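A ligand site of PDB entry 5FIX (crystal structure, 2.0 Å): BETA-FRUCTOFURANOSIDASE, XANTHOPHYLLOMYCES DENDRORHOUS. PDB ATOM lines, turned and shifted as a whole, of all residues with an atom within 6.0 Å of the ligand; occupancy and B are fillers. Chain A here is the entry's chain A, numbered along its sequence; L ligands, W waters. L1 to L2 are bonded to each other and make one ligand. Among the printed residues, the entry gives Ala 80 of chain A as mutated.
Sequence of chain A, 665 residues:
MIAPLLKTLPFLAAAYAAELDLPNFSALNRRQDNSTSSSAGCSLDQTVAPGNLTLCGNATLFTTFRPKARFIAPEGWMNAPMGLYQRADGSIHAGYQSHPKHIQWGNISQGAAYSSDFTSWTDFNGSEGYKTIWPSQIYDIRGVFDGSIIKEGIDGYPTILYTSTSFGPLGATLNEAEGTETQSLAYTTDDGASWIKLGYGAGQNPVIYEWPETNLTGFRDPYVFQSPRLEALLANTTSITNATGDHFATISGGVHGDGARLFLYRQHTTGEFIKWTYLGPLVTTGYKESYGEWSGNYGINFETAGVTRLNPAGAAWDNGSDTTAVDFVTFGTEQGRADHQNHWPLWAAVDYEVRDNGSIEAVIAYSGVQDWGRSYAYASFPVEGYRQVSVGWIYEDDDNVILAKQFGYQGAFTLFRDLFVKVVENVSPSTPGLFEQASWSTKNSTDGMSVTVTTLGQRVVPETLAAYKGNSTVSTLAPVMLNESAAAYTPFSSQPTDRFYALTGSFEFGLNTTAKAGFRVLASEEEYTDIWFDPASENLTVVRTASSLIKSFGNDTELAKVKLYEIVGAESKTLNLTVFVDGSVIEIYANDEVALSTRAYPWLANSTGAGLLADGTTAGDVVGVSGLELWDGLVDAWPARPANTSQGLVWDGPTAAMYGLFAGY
The backbone carbonyl oxygen (O) of Gln 97 is in hydrogen-bond range of the backbone NH (N) of Asn 79 (2.9 Å).
N of Gln 97 lies within hydrogen-bond range of O of Ala 80 (2.8 Å).
The side-chain amide nitrogen of Gln 97 lies within hydrogen-bond range of the backbone carbonyl oxygen of Val 144 (2.8 Å).
The backbone NH (N) of Thr 304 sits at hydrogen-bond distance from the side-chain carboxylate (OD2) of Asp 221, at 2.8 Å.
OE2 of Glu 334 is in salt-bridge range of NH2 of Arg 220.
OE2 of Glu 303 lies within salt-bridge range of NH2 of Arg 220.
The side-chain carboxylate (OE1) of Glu 303 is in hydrogen-bond range of the side-chain hydroxyl (OH) of Tyr 376, at 2.6 Å.
N of Val 144 sits at hydrogen-bond distance from O of Ile 108, at 2.8 Å.
Residues that only touch the ligand: Phe 145, Tyr 376 and Ile 108.
Hydrophobic or aromatic side chains that line the ligand: Trp 105, Ile 108, Phe 145, His 343 and Tyr 376.
Of the 22 residues printed, 12 come within 4 Å of the ligand.
Along chain A the residues within 4 Å of the ligand span positions 79 to 376.
An oxygen (O6) of LG2 L2 lies within hydrogen-bond range of the side-chain amide oxygen of Gln 97 (2.5 Å).
OD2 of Asp 221 lies within hydrogen-bond range of O3 of LG2 L2 (2.6 Å).
OE1 of Glu 334 lies within hydrogen-bond range of O2 of LIG L1 (2.6 Å).
NE1 of Trp 105 is in hydrogen-bond range of O6 of LG2 L2.
O1 of LIG L1 is in hydrogen-bond range of OE2 of Glu 303, at 2.9 Å.
NE of Arg 220 lies within hydrogen-bond range of O3 of LG2 L2, 3.0 Å away.
An oxygen (O6) of LG2 L2 is in hydrogen-bond range of the side-chain amide nitrogen (ND2) of Asn 79 (3.0 Å).
The backbone NH (N) of Asp 146 sits at hydrogen-bond distance from an oxygen (O4) of LG2 L2 (3.2 Å).
An oxygen (O1) of LIG L1 lies close to a ring nitrogen (NE2) of His 343 (3.2 Å).
Water W1 lies within hydrogen-bond range of O3 of LIG L1 (2.6 Å) and O of Leu 170 (2.7 Å).
Water W5 bridges O1 of LG2 L2 and ND2 of Asn 79.
Water W4 lies within hydrogen-bond range of OE2 of Glu 334 (2.7 Å), N of Ala 172 (3.0 Å), NH2 of Arg 220 (3.1 Å) and O3 of LIG L1 (3.1 Å).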
ATOM      1  N   ASN A  79      12.301 -17.375   8.498  1.00  0.00           N
ATOM      2  CA  ASN A  79      12.928 -18.682   8.497  1.00  0.00           C
ATOM      3  C   ASN A  79      14.455 -18.567   8.690  1.00  0.00           C
ATOM      4  O   ASN A  79      14.873 -18.037   9.728  1.00  0.00           O
ATOM      5  CB  ASN A  79      12.426 -19.616   7.335  1.00  0.00           C
ATOM      6  CG  ASN A  79      12.609 -19.063   5.923  1.00  0.00           C
ATOM      7  OD1 ASN A  79      12.005 -18.063   5.539  1.00  0.00           O
ATOM      8  ND2 ASN A  79      13.412 -19.758   5.122  1.00  0.00           N
ATOM      9  N   ALA A  80      15.263 -19.045   7.749  1.00  0.00           N
ATOM     10  CA  ALA A  80      16.702 -19.250   7.931  1.00  0.00           C
ATOM     11  C   ALA A  80      17.469 -17.995   8.361  1.00  0.00           C
ATOM     12  O   ALA A  80      17.264 -16.926   7.804  1.00  0.00           O
ATOM     13  CB  ALA A  80      17.301 -19.762   6.634  1.00  0.00           C
ATOM     14  N   GLN A  97      15.812 -14.700   6.787  1.00  0.00           N
ATOM     15  CA  GLN A  97      14.786 -14.772   5.775  1.00  0.00           C
ATOM     16  C   GLN A  97      13.458 -14.251   6.407  1.00  0.00           C
ATOM     17  O   GLN A  97      13.058 -14.751   7.461  1.00  0.00           O
ATOM     18  CB  GLN A  97      14.620 -16.214   5.303  1.00  0.00           C
ATOM     19  CG  GLN A  97      15.827 -16.733   4.547  1.00  0.00           C
ATOM     20  CD  GLN A  97      15.864 -16.245   3.122  1.00  0.00           C
ATOM     21  OE1 GLN A  97      15.263 -16.870   2.238  1.00  0.00           O
ATOM     22  NE2 GLN A  97      16.598 -15.155   2.873  1.00  0.00           N
ATOM     23  N   TRP A 105       5.687 -18.011   3.863  1.00  0.00           N
ATOM     24  CA  TRP A 105       6.855 -17.577   3.099  1.00  0.00           C
ATOM     25  C   TRP A 105       6.477 -16.834   1.806  1.00  0.00           C
ATOM     26  O   TRP A 105       5.462 -17.132   1.182  1.00  0.00           O
ATOM     27  CB  TRP A 105       7.684 -18.830   2.787  1.00  0.00           C
ATOM     28  CG  TRP A 105       8.981 -18.697   2.039  1.00  0.00           C
ATOM     29  CD1 TRP A 105      10.231 -18.664   2.572  1.00  0.00           C
ATOM     30  CD2 TRP A 105       9.146 -18.692   0.620  1.00  0.00           C
ATOM     31  NE1 TRP A 105      11.171 -18.586   1.576  1.00  0.00           N
ATOM     32  CE2 TRP A 105      10.527 -18.627   0.361  1.00  0.00           C
ATOM     33  CE3 TRP A 105       8.251 -18.742  -0.467  1.00  0.00           C
ATOM     34  CZ2 TRP A 105      11.053 -18.598  -0.928  1.00  0.00           C
ATOM     35  CZ3 TRP A 105       8.770 -18.727  -1.749  1.00  0.00           C
ATOM     36  CH2 TRP A 105      10.155 -18.655  -1.978  1.00  0.00           C
ATOM     37  N   ILE A 108      10.854 -13.212  -0.385  1.00  0.00           N
ATOM     38  CA  ILE A 108      11.688 -13.445   0.782  1.00  0.00           C
ATOM     39  C   ILE A 108      12.846 -12.434   0.771  1.00  0.00           C
ATOM     40  O   ILE A 108      13.442 -12.181  -0.275  1.00  0.00           O
ATOM     41  CB  ILE A 108      12.075 -14.928   0.945  1.00  0.00           C
ATOM     42  CG1 ILE A 108      12.364 -15.268   2.421  1.00  0.00           C
ATOM     43  CG2 ILE A 108      13.247 -15.322   0.045  1.00  0.00           C
ATOM     44  CD1 ILE A 108      11.141 -15.236   3.342  1.00  0.00           C
ATOM     45  N   VAL A 144      15.194 -13.022  -2.340  1.00  0.00           N
ATOM     46  CA  VAL A 144      16.535 -12.923  -1.831  1.00  0.00           C
ATOM     47  C   VAL A 144      16.709 -14.044  -0.809  1.00  0.00           C
ATOM     48  O   VAL A 144      16.334 -13.907   0.365  1.00  0.00           O
ATOM     49  CB  VAL A 144      16.789 -11.532  -1.186  1.00  0.00           C
ATOM     50  CG1 VAL A 144      18.150 -11.473  -0.505  1.00  0.00           C
ATOM     51  CG2 VAL A 144      16.682 -10.458  -2.248  1.00  0.00           C
ATOM     52  N   PHE A 145      17.263 -15.160  -1.271  1.00  0.00           N
ATOM     53  CA  PHE A 145      17.440 -16.374  -0.474  1.00  0.00           C
ATOM     54  C   PHE A 145      18.703 -16.222   0.400  1.00  0.00           C
ATOM     55  O   PHE A 145      19.264 -15.130   0.513  1.00  0.00           O
ATOM     56  CB  PHE A 145      17.545 -17.613  -1.397  1.00  0.00           C
ATOM     57  CG  PHE A 145      16.225 -18.117  -1.938  1.00  0.00           C
ATOM     58  CD1 PHE A 145      15.134 -17.295  -2.157  1.00  0.00           C
ATOM     59  CD2 PHE A 145      16.128 -19.459  -2.308  1.00  0.00           C
ATOM     60  CE1 PHE A 145      13.958 -17.784  -2.704  1.00  0.00           C
ATOM     61  CE2 PHE A 145      14.950 -19.970  -2.857  1.00  0.00           C
ATOM     62  CZ  PHE A 145      13.862 -19.128  -3.050  1.00  0.00           C
ATOM     63  N   ASP A 146      19.087 -17.301   1.085  1.00  0.00           N
ATOM     64  CA  ASP A 146      20.226 -17.318   2.018  1.00  0.00           C
ATOM     65  C   ASP A 146      21.521 -16.831   1.362  1.00  0.00           C
ATOM     66  O   ASP A 146      21.733 -16.993   0.157  1.00  0.00           O
ATOM     67  CB  ASP A 146      20.395 -18.758   2.516  1.00  0.00           C
ATOM     68  CG  ASP A 146      21.345 -18.899   3.705  1.00  0.00           C
ATOM     69  OD1 ASP A 146      21.680 -17.924   4.412  1.00  0.00           O
ATOM     70  OD2 ASP A 146      21.761 -20.075   3.938  1.00  0.00           O
ATOM     71  N   THR A 163      21.817 -16.128  -2.709  1.00  0.00           N
ATOM     72  CA  THR A 163      21.078 -16.716  -3.817  1.00  0.00           C
ATOM     73  C   THR A 163      19.974 -15.776  -4.289  1.00  0.00           C
ATOM     74  O   THR A 163      19.029 -15.475  -3.551  1.00  0.00           O
ATOM     75  CB  THR A 163      20.525 -18.093  -3.476  1.00  0.00           C
ATOM     76  OG1 THR A 163      21.606 -18.987  -3.184  1.00  0.00           O
ATOM     77  CG2 THR A 163      19.700 -18.632  -4.624  1.00  0.00           C
ATOM     78  N   LEU A 170      11.004 -24.146  -9.005  1.00  0.00           N
ATOM     79  CA  LEU A 170      12.103 -24.092  -8.068  1.00  0.00           C
ATOM     80  C   LEU A 170      11.797 -25.103  -6.959  1.00  0.00           C
ATOM     81  O   LEU A 170      10.782 -24.974  -6.255  1.00  0.00           O
ATOM     82  CB  LEU A 170      12.239 -22.668  -7.501  1.00  0.00           C
ATOM     83  CG  LEU A 170      13.555 -22.295  -6.761  1.00  0.00           C
ATOM     84  CD1 LEU A 170      13.641 -20.787  -6.558  1.00  0.00           C
ATOM     85  CD2 LEU A 170      13.686 -23.017  -5.424  1.00  0.00           C
ATOM     86  N   GLY A 171      12.649 -26.115  -6.835  1.00  0.00           N
ATOM     87  CA  GLY A 171      12.512 -27.096  -5.774  1.00  0.00           C
ATOM     88  C   GLY A 171      13.122 -28.417  -6.132  1.00  0.00           C
ATOM     89  O   GLY A 171      13.193 -28.785  -7.307  1.00  0.00           O
ATOM     90  N   ALA A 172      13.535 -29.150  -5.098  1.00  0.00           N
ATOM     91  CA  ALA A 172      14.206 -30.423  -5.255  1.00  0.00           C
ATOM     92  C   ALA A 172      13.328 -31.506  -5.891  1.00  0.00           C
ATOM     93  O   ALA A 172      13.851 -32.417  -6.537  1.00  0.00           O
ATOM     94  CB  ALA A 172      14.720 -30.890  -3.899  1.00  0.00           C
ATOM     95  N   ARG A 220      21.885 -23.307  -4.384  1.00  0.00           N
ATOM     96  CA  ARG A 220      21.686 -22.170  -3.501  1.00  0.00           C
ATOM     97  C   ARG A 220      22.482 -22.211  -2.206  1.00  0.00           C
ATOM     98  O   ARG A 220      23.171 -23.198  -1.920  1.00  0.00           O
ATOM     99  CB  ARG A 220      20.184 -22.046  -3.169  1.00  0.00           C
ATOM    100  CG  ARG A 220      19.545 -23.234  -2.469  1.00  0.00           C
ATOM    101  CD  ARG A 220      18.138 -22.886  -1.973  1.00  0.00           C
ATOM    102  NE  ARG A 220      17.377 -24.073  -1.595  1.00  0.00           N
ATOM    103  CZ  ARG A 220      16.810 -24.923  -2.456  1.00  0.00           C
ATOM    104  NH1 ARG A 220      16.869 -24.713  -3.772  1.00  0.00           N
ATOM    105  NH2 ARG A 220      16.188 -25.999  -2.016  1.00  0.00           N
ATOM    106  N   ASP A 221      22.358 -21.120  -1.458  1.00  0.00           N
ATOM    107  CA  ASP A 221      22.886 -20.971  -0.110  1.00  0.00           C
ATOM    108  C   ASP A 221      24.410 -20.928  -0.111  1.00  0.00           C
ATOM    109  O   ASP A 221      25.061 -21.745   0.563  1.00  0.00           O
ATOM    110  CB  ASP A 221      22.347 -22.055   0.838  1.00  0.00           C
ATOM    111  CG  ASP A 221      20.813 -22.134   0.846  1.00  0.00           C
ATOM    112  OD1 ASP A 221      20.164 -21.158   0.401  1.00  0.00           O
ATOM    113  OD2 ASP A 221      20.297 -23.178   1.271  1.00  0.00           O
ATOM    114  N   PHE A 302      20.882 -30.973  -0.589  1.00  0.00           N
ATOM    115  CA  PHE A 302      21.432 -30.223   0.553  1.00  0.00           C
ATOM    116  C   PHE A 302      20.960 -28.790   0.514  1.00  0.00           C
ATOM    117  O   PHE A 302      20.697 -28.226  -0.541  1.00  0.00           O
ATOM    118  CB  PHE A 302      22.972 -30.176   0.559  1.00  0.00           C
ATOM    119  CG  PHE A 302      23.657 -31.492   0.866  1.00  0.00           C
ATOM    120  CD1 PHE A 302      23.090 -32.449   1.706  1.00  0.00           C
ATOM    121  CD2 PHE A 302      24.920 -31.732   0.345  1.00  0.00           C
ATOM    122  CE1 PHE A 302      23.768 -33.645   1.969  1.00  0.00           C
ATOM    123  CE2 PHE A 302      25.601 -32.919   0.613  1.00  0.00           C
ATOM    124  CZ  PHE A 302      25.027 -33.865   1.438  1.00  0.00           C
ATOM    125  N   GLU A 303      20.895 -28.194   1.702  1.00  0.00           N
ATOM    126  CA  GLU A 303      20.598 -26.791   1.872  1.00  0.00           C
ATOM    127  C   GLU A 303      21.431 -26.226   3.010  1.00  0.00           C
ATOM    128  O   GLU A 303      21.858 -26.968   3.899  1.00  0.00           O
ATOM    129  CB  GLU A 303      19.110 -26.587   2.202  1.00  0.00           C
ATOM    130  CG  GLU A 303      18.148 -27.139   1.163  1.00  0.00           C
ATOM    131  CD  GLU A 303      16.703 -26.897   1.550  1.00  0.00           C
ATOM    132  OE1 GLU A 303      16.279 -27.326   2.640  1.00  0.00           O
ATOM    133  OE2 GLU A 303      15.971 -26.311   0.740  1.00  0.00           O
ATOM    134  N   THR A 304      21.627 -24.916   2.966  1.00  0.00           N
ATOM    135  CA  THR A 304      22.320 -24.124   3.989  1.00  0.00           C
ATOM    136  C   THR A 304      23.604 -24.776   4.498  1.00  0.00           C
ATOM    137  O   THR A 304      23.892 -24.717   5.676  1.00  0.00           O
ATOM    138  CB  THR A 304      21.405 -23.728   5.187  1.00  0.00           C
ATOM    139  OG1 THR A 304      21.189 -24.856   6.065  1.00  0.00           O
ATOM    140  CG2 THR A 304      20.070 -23.187   4.718  1.00  0.00           C
ATOM    141  N   GLU A 334      16.938 -32.592   2.536  1.00  0.00           N
ATOM    142  CA  GLU A 334      15.526 -32.613   2.209  1.00  0.00           C
ATOM    143  C   GLU A 334      15.085 -33.994   1.703  1.00  0.00           C
ATOM    144  O   GLU A 334      15.837 -34.663   0.997  1.00  0.00           O
ATOM    145  CB  GLU A 334      15.218 -31.660   1.055  1.00  0.00           C
ATOM    146  CG  GLU A 334      15.789 -30.257   1.158  1.00  0.00           C
ATOM    147  CD  GLU A 334      14.980 -29.310   0.298  1.00  0.00           C
ATOM    148  OE1 GLU A 334      13.915 -28.860   0.791  1.00  0.00           O
ATOM    149  OE2 GLU A 334      15.398 -29.062  -0.850  1.00  0.00           O
ATOM    150  N   HIS A 343      12.973 -32.507   6.791  1.00  0.00           N
ATOM    151  CA  HIS A 343      14.243 -31.784   6.957  1.00  0.00           C
ATOM    152  C   HIS A 343      15.104 -32.293   8.115  1.00  0.00           C
ATOM    153  O   HIS A 343      14.649 -32.327   9.260  1.00  0.00           O
ATOM    154  CB  HIS A 343      13.941 -30.311   7.220  1.00  0.00           C
ATOM    155  CG  HIS A 343      13.729 -29.508   5.979  1.00  0.00           C
ATOM    156  ND1 HIS A 343      12.962 -28.359   5.964  1.00  0.00           N
ATOM    157  CD2 HIS A 343      14.164 -29.670   4.706  1.00  0.00           C
ATOM    158  CE1 HIS A 343      12.952 -27.849   4.748  1.00  0.00           C
ATOM    159  NE2 HIS A 343      13.682 -28.624   3.966  1.00  0.00           N
ATOM    160  N   TYR A 376      16.110 -26.179  11.820  1.00  0.00           N
ATOM    161  CA  TYR A 376      16.717 -26.366  10.511  1.00  0.00           C
ATOM    162  C   TYR A 376      17.483 -25.099  10.134  1.00  0.00           C
ATOM    163  O   TYR A 376      17.360 -24.083  10.803  1.00  0.00           O
ATOM    164  CB  TYR A 376      15.634 -26.630   9.471  1.00  0.00           C
ATOM    165  CG  TYR A 376      16.116 -27.184   8.149  1.00  0.00           C
ATOM    166  CD1 TYR A 376      16.761 -28.406   8.067  1.00  0.00           C
ATOM    167  CD2 TYR A 376      15.900 -26.488   6.954  1.00  0.00           C
ATOM    168  CE1 TYR A 376      17.181 -28.932   6.861  1.00  0.00           C
ATOM    169  CE2 TYR A 376      16.324 -26.995   5.733  1.00  0.00           C
ATOM    170  CZ  TYR A 376      16.950 -28.226   5.680  1.00  0.00           C
ATOM    171  OH  TYR A 376      17.368 -28.762   4.494  1.00  0.00           O
ATOM    172  N   ALA A 377      18.267 -25.193   9.068  1.00  0.00           N
ATOM    173  CA  ALA A 377      18.909 -24.032   8.440  1.00  0.00           C
ATOM    174  C   ALA A 377      19.900 -23.412   9.380  1.00  0.00           C
ATOM    175  O   ALA A 377      19.926 -22.203   9.560  1.00  0.00           O
ATOM    176  CB  ALA A 377      17.864 -23.016   7.966  1.00  0.00           C
ATOM    177  N   TRP A 393      17.061 -22.073  12.889  1.00  0.00           N
ATOM    178  CA  TRP A 393      15.680 -21.602  12.881  1.00  0.00           C
ATOM    179  C   TRP A 393      14.787 -22.671  13.472  1.00  0.00           C
ATOM    180  O   TRP A 393      14.867 -23.823  13.057  1.00  0.00           O
ATOM    181  CB  TRP A 393      15.282 -21.291  11.437  1.00  0.00           C
ATOM    182  CG  TRP A 393      13.801 -21.336  11.087  1.00  0.00           C
ATOM    183  CD1 TRP A 393      12.799 -20.554  11.586  1.00  0.00           C
ATOM    184  CD2 TRP A 393      13.195 -22.155  10.083  1.00  0.00           C
ATOM    185  NE1 TRP A 393      11.607 -20.858  10.992  1.00  0.00           N
ATOM    186  CE2 TRP A 393      11.821 -21.831  10.058  1.00  0.00           C
ATOM    187  CE3 TRP A 393      13.682 -23.138   9.220  1.00  0.00           C
ATOM    188  CZ2 TRP A 393      10.930 -22.460   9.182  1.00  0.00           C
ATOM    189  CZ3 TRP A 393      12.797 -23.763   8.356  1.00  0.00           C
ATOM    190  CH2 TRP A 393      11.432 -23.428   8.348  1.00  0.00           C
HETATM  191  C1  LIG L   1      13.533 -23.432   1.781  1.00  0.00           C
HETATM  192  C2  LIG L   1      13.047 -24.895   1.673  1.00  0.00           C
HETATM  193  C3  LIG L   1      13.129 -25.404   0.248  1.00  0.00           C
HETATM  194  C4  LIG L   1      12.410 -24.477  -0.697  1.00  0.00           C
HETATM  195  C5  LIG L   1      12.982 -23.076  -0.569  1.00  0.00           C
HETATM  196  C6  LIG L   1      12.227 -22.083  -1.438  1.00  0.00           C
HETATM  197  O1  LIG L   1      13.809 -25.761   2.522  1.00  0.00           O
HETATM  198  O2  LIG L   1      12.573 -26.717   0.188  1.00  0.00           O
HETATM  199  O3  LIG L   1      12.573 -24.954  -2.033  1.00  0.00           O
HETATM  200  O4  LIG L   1      12.906 -22.625   0.785  1.00  0.00           O
HETATM  201  O5  LIG L   1      10.829 -22.086  -1.088  1.00  0.00           O
HETATM  202  C1  LG2 L   2      16.068 -23.577   3.827  1.00  0.00           C
HETATM  203  C2  LG2 L   2      15.779 -22.688   2.605  1.00  0.00           C
HETATM  204  C3  LG2 L   2      17.122 -22.284   1.985  1.00  0.00           C
HETATM  205  C4  LG2 L   2      16.727 -21.065   1.180  1.00  0.00           C
HETATM  206  C5  LG2 L   2      15.708 -20.407   2.112  1.00  0.00           C
HETATM  207  C6  LG2 L   2      14.571 -19.693   1.379  1.00  0.00           C
HETATM  208  O1  LG2 L   2      14.881 -24.146   4.373  1.00  0.00           O
HETATM  209  O2  LG2 L   2      14.958 -23.332   1.605  1.00  0.00           O
HETATM  210  O3  LG2 L   2      17.746 -23.341   1.240  1.00  0.00           O
HETATM  211  O4  LG2 L   2      17.815 -20.177   0.892  1.00  0.00           O
HETATM  212  O5  LG2 L   2      15.231 -21.432   2.979  1.00  0.00           O
HETATM  213  O6  LG2 L   2      13.805 -18.903   2.308  1.00  0.00           O
HETATM  214  O   HOH W   1      10.504 -24.599  -3.592  1.00  0.00           O
HETATM  215  O   HOH W   2       9.125 -21.987  -3.137  1.00  0.00           O
HETATM  216  O   HOH W   3       9.928 -27.229  -0.384  1.00  0.00           O
HETATM  217  O   HOH W   4      13.726 -27.762  -2.491  1.00  0.00           O
HETATM  218  O   HOH W   5      14.457 -22.241   6.117  1.00  0.00           O
HETATM  219  O   HOH W   6       9.819 -22.031   1.693  1.00  0.00           O
